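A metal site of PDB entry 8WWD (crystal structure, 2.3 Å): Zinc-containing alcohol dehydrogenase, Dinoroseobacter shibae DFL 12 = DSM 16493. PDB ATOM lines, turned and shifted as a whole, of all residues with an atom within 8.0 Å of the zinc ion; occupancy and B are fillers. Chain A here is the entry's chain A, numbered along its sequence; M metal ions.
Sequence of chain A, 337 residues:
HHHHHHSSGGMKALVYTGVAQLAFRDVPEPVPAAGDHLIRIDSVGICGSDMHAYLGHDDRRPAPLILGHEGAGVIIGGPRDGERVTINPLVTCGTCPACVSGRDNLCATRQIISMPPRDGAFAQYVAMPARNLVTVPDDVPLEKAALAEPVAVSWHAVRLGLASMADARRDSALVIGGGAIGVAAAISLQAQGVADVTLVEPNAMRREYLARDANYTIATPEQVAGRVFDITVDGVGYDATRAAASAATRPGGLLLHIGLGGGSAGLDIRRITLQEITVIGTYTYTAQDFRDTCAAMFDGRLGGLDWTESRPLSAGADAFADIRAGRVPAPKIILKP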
ATOM      1  N   VAL A  91     -10.305  22.040  10.527  1.00  0.00           N
ATOM      2  CA  VAL A  91     -11.063  22.763  11.588  1.00  0.00           C
ATOM      3  C   VAL A  91     -12.532  22.408  11.461  1.00  0.00           C
ATOM      4  O   VAL A  91     -13.110  22.600  10.352  1.00  0.00           O
ATOM      5  CB  VAL A  91     -10.818  24.276  11.510  1.00  0.00           C
ATOM      6  CG1 VAL A  91     -11.589  25.022  12.596  1.00  0.00           C
ATOM      7  CG2 VAL A  91      -9.348  24.573  11.611  1.00  0.00           C
ATOM      8  N   THR A  92     -13.111  21.893  12.545  1.00  0.00           N
ATOM      9  CA  THR A  92     -14.481  21.328  12.592  1.00  0.00           C
ATOM     10  C   THR A  92     -15.321  22.112  13.600  1.00  0.00           C
ATOM     11  O   THR A  92     -14.751  22.742  14.522  1.00  0.00           O
ATOM     12  CB  THR A  92     -14.399  19.827  12.861  1.00  0.00           C
ATOM     13  OG1 THR A  92     -13.859  19.619  14.166  1.00  0.00           O
ATOM     14  CG2 THR A  92     -13.507  19.101  11.883  1.00  0.00           C
ATOM     15  N   CYS A  93     -16.640  22.115  13.444  1.00  0.00           N
ATOM     16  CA  CYS A  93     -17.545  23.015  14.200  1.00  0.00           C
ATOM     17  C   CYS A  93     -17.806  22.440  15.610  1.00  0.00           C
ATOM     18  O   CYS A  93     -18.122  23.238  16.529  1.00  0.00           O
ATOM     19  CB  CYS A  93     -18.825  23.265  13.407  1.00  0.00           C
ATOM     20  SG  CYS A  93     -20.048  21.999  13.585  1.00  0.00           S
ATOM     21  N   GLY A  94     -17.758  21.123  15.774  1.00  0.00           N
ATOM     22  CA  GLY A  94     -18.030  20.450  17.062  1.00  0.00           C
ATOM     23  C   GLY A  94     -19.523  20.287  17.417  1.00  0.00           C
ATOM     24  O   GLY A  94     -19.787  19.584  18.427  1.00  0.00           O
ATOM     25  N   THR A  95     -20.471  20.853  16.657  1.00  0.00           N
ATOM     26  CA  THR A  95     -21.923  20.831  17.033  1.00  0.00           C
ATOM     27  C   THR A  95     -22.867  20.343  15.925  1.00  0.00           C
ATOM     28  O   THR A  95     -24.068  20.273  16.231  1.00  0.00           O
ATOM     29  CB  THR A  95     -22.426  22.207  17.477  1.00  0.00           C
ATOM     30  OG1 THR A  95     -22.320  23.088  16.357  1.00  0.00           O
ATOM     31  CG2 THR A  95     -21.650  22.775  18.637  1.00  0.00           C
ATOM     32  N   CYS A  96     -22.377  19.996  14.731  1.00  0.00           N
ATOM     33  CA  CYS A  96     -23.203  19.449  13.630  1.00  0.00           C
ATOM     34  C   CYS A  96     -23.466  17.958  13.886  1.00  0.00           C
ATOM     35  O   CYS A  96     -22.845  17.336  14.745  1.00  0.00           O
ATOM     36  CB  CYS A  96     -22.557  19.728  12.275  1.00  0.00           C
ATOM     37  SG  CYS A  96     -21.154  18.727  11.896  1.00  0.00           S
ATOM     38  N   PRO A  97     -24.414  17.317  13.176  1.00  0.00           N
ATOM     39  CA  PRO A  97     -24.655  15.881  13.365  1.00  0.00           C
ATOM     40  C   PRO A  97     -23.414  14.993  13.164  1.00  0.00           C
ATOM     41  O   PRO A  97     -23.238  13.989  13.855  1.00  0.00           O
ATOM     42  CB  PRO A  97     -25.722  15.586  12.306  1.00  0.00           C
ATOM     43  CG  PRO A  97     -26.453  16.908  12.144  1.00  0.00           C
ATOM     44  CD  PRO A  97     -25.345  17.945  12.228  1.00  0.00           C
ATOM     45  N   ALA A  98     -22.589  15.298  12.184  1.00  0.00           N
ATOM     46  CA  ALA A  98     -21.368  14.489  11.975  1.00  0.00           C
ATOM     47  C   ALA A  98     -20.467  14.641  13.202  1.00  0.00           C
ATOM     48  O   ALA A  98     -19.980  13.638  13.709  1.00  0.00           O
ATOM     49  CB  ALA A  98     -20.718  14.857  10.660  1.00  0.00           C
ATOM     50  N   CYS A  99     -20.284  15.856  13.717  1.00  0.00           N
ATOM     51  CA  CYS A  99     -19.370  16.137  14.855  1.00  0.00           C
ATOM     52  C   CYS A  99     -19.934  15.457  16.101  1.00  0.00           C
ATOM     53  O   CYS A  99     -19.184  14.734  16.788  1.00  0.00           O
ATOM     54  CB  CYS A  99     -19.155  17.635  15.044  1.00  0.00           C
ATOM     55  SG  CYS A  99     -18.159  18.395  13.759  1.00  0.00           S
ATOM     56  N   VAL A 100     -21.235  15.619  16.367  1.00  0.00           N
ATOM     57  CA  VAL A 100     -21.912  15.047  17.559  1.00  0.00           C
ATOM     58  C   VAL A 100     -21.764  13.514  17.511  1.00  0.00           C
ATOM     59  O   VAL A 100     -21.582  12.913  18.564  1.00  0.00           O
ATOM     60  CB  VAL A 100     -23.391  15.487  17.638  1.00  0.00           C
ATOM     61  CG1 VAL A 100     -24.238  14.556  18.486  1.00  0.00           C
ATOM     62  CG2 VAL A 100     -23.513  16.930  18.119  1.00  0.00           C
ATOM     63  N   ARG A 103     -17.716  11.839  14.126  1.00  0.00           N
ATOM     64  CA  ARG A 103     -17.166  11.770  12.743  1.00  0.00           C
ATOM     65  C   ARG A 103     -16.893  13.204  12.266  1.00  0.00           C
ATOM     66  O   ARG A 103     -17.266  13.569  11.130  1.00  0.00           O
ATOM     67  CB  ARG A 103     -18.117  10.978  11.864  1.00  0.00           C
ATOM     68  CG  ARG A 103     -18.256   9.519  12.290  1.00  0.00           C
ATOM     69  CD  ARG A 103     -19.027   8.692  11.281  1.00  0.00           C
ATOM     70  NE  ARG A 103     -18.263   8.331  10.099  1.00  0.00           N
ATOM     71  CZ  ARG A 103     -18.774   7.691   9.046  1.00  0.00           C
ATOM     72  NH1 ARG A 103     -20.035   7.301   9.048  1.00  0.00           N
ATOM     73  NH2 ARG A 103     -18.004   7.413   8.005  1.00  0.00           N
ATOM     74  N   ASP A 104     -16.193  13.981  13.085  1.00  0.00           N
ATOM     75  CA  ASP A 104     -15.928  15.421  12.833  1.00  0.00           C
ATOM     76  C   ASP A 104     -15.132  15.612  11.529  1.00  0.00           C
ATOM     77  O   ASP A 104     -15.200  16.711  10.987  1.00  0.00           O
ATOM     78  CB  ASP A 104     -15.262  16.040  14.045  1.00  0.00           C
ATOM     79  CG  ASP A 104     -14.128  15.188  14.564  1.00  0.00           C
ATOM     80  OD1 ASP A 104     -13.058  15.218  13.915  1.00  0.00           O
ATOM     81  OD2 ASP A 104     -14.327  14.485  15.595  1.00  0.00           O
ATOM     82  N   ASN A 105     -14.458  14.574  11.011  1.00  0.00           N
ATOM     83  CA  ASN A 105     -13.854  14.588   9.641  1.00  0.00           C
ATOM     84  C   ASN A 105     -14.925  14.881   8.581  1.00  0.00           C
ATOM     85  O   ASN A 105     -14.546  15.321   7.494  1.00  0.00           O
ATOM     86  CB  ASN A 105     -13.160  13.280   9.302  1.00  0.00           C
ATOM     87  CG  ASN A 105     -14.098  12.082   9.297  1.00  0.00           C
ATOM     88  OD1 ASN A 105     -14.958  11.962  10.161  1.00  0.00           O
ATOM     89  ND2 ASN A 105     -13.943  11.195   8.319  1.00  0.00           N
ATOM     90  N   LEU A 106     -16.208  14.629   8.877  1.00  0.00           N
ATOM     91  CA  LEU A 106     -17.363  14.862   7.963  1.00  0.00           C
ATOM     92  C   LEU A 106     -18.161  16.082   8.397  1.00  0.00           C
ATOM     93  O   LEU A 106     -19.301  16.233   7.919  1.00  0.00           O
ATOM     94  CB  LEU A 106     -18.244  13.611   7.985  1.00  0.00           C
ATOM     95  CG  LEU A 106     -17.515  12.335   7.554  1.00  0.00           C
ATOM     96  CD1 LEU A 106     -18.475  11.150   7.564  1.00  0.00           C
ATOM     97  CD2 LEU A 106     -16.868  12.521   6.198  1.00  0.00           C
ATOM     98  N   CYS A 107     -17.593  16.951   9.236  1.00  0.00           N
ATOM     99  CA  CYS A 107     -18.226  18.217   9.673  1.00  0.00           C
ATOM    100  C   CYS A 107     -18.770  18.969   8.464  1.00  0.00           C
ATOM    101  O   CYS A 107     -18.027  19.183   7.485  1.00  0.00           O
ATOM    102  CB  CYS A 107     -17.239  19.108  10.427  1.00  0.00           C
ATOM    103  SG  CYS A 107     -17.960  20.702  10.753  1.00  0.00           S
ATOM    104  N   ALA A 108     -20.023  19.417   8.544  1.00  0.00           N
ATOM    105  CA  ALA A 108     -20.727  20.099   7.429  1.00  0.00           C
ATOM    106  C   ALA A 108     -20.041  21.426   7.096  1.00  0.00           C
ATOM    107  O   ALA A 108     -20.204  21.866   5.971  1.00  0.00           O
ATOM    108  CB  ALA A 108     -22.199  20.276   7.760  1.00  0.00           C
ATOM    109  N   THR A 109     -19.306  22.060   8.027  1.00  0.00           N
ATOM    110  CA  THR A 109     -18.595  23.345   7.737  1.00  0.00           C
ATOM    111  C   THR A 109     -17.080  23.167   7.897  1.00  0.00           C
ATOM    112  O   THR A 109     -16.389  24.154   8.123  1.00  0.00           O
ATOM    113  CB  THR A 109     -19.168  24.493   8.569  1.00  0.00           C
ATOM    114  OG1 THR A 109     -19.037  24.114   9.929  1.00  0.00           O
ATOM    115  CG2 THR A 109     -20.622  24.778   8.260  1.00  0.00           C
ATOM    116  N   ARG A 110     -16.563  21.960   7.665  1.00  0.00           N
ATOM    117  CA  ARG A 110     -15.122  21.661   7.831  1.00  0.00           C
ATOM    118  C   ARG A 110     -14.314  22.594   6.918  1.00  0.00           C
ATOM    119  O   ARG A 110     -14.673  22.785   5.719  1.00  0.00           O
ATOM    120  CB  ARG A 110     -14.829  20.195   7.548  1.00  0.00           C
ATOM    121  CG  ARG A 110     -15.057  19.800   6.100  1.00  0.00           C
ATOM    122  CD  ARG A 110     -14.921  18.306   5.915  1.00  0.00           C
ATOM    123  NE  ARG A 110     -14.809  17.970   4.499  1.00  0.00           N
ATOM    124  CZ  ARG A 110     -15.177  16.823   3.947  1.00  0.00           C
ATOM    125  NH1 ARG A 110     -15.684  15.855   4.704  1.00  0.00           N
ATOM    126  NH2 ARG A 110     -15.036  16.642   2.647  1.00  0.00           N
HETATM  127 ZN    ZN M   1     -19.340  20.045  12.528  1.00  0.00          ZN
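SG of Cys 107 sits close to N of Thr 109 (3.3 Å).
The side-chain sulfur (SG) of Cys 93 sits close to the backbone NH (N) of Thr 95, at 3.3 Å.
The side-chain sulfur (SG) of Cys 107 lies close to the backbone NH (N) of Arg 110, 3.6 Å away.
SG of Cys 96 lies close to N of Ala 98 (3.7 Å).
The side-chain sulfur (SG) of Cys 99 sits close to the backbone NH (N) of Gly 94, at 3.4 Å.
N of Ala 108 lies close to SG of Cys 96, at 3.6 Å.
Merely in contact with the zinc ion: Gly 94.
Within 4 Å of the zinc ion: Cys 93, Gly 94, Cys 96, Cys 99 and Cys 107.
The zinc ion is bound by the side-chain sulfur of Cys 96 (2.3 Å), the side-chain sulfur of Cys 93 (2.3 Å), the side-chain sulfur of Cys 107 (2.3 Å) and the side-chain sulfur of Cys 99 (2.4 Å).
The zinc ion has four donor atoms within binding distance.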
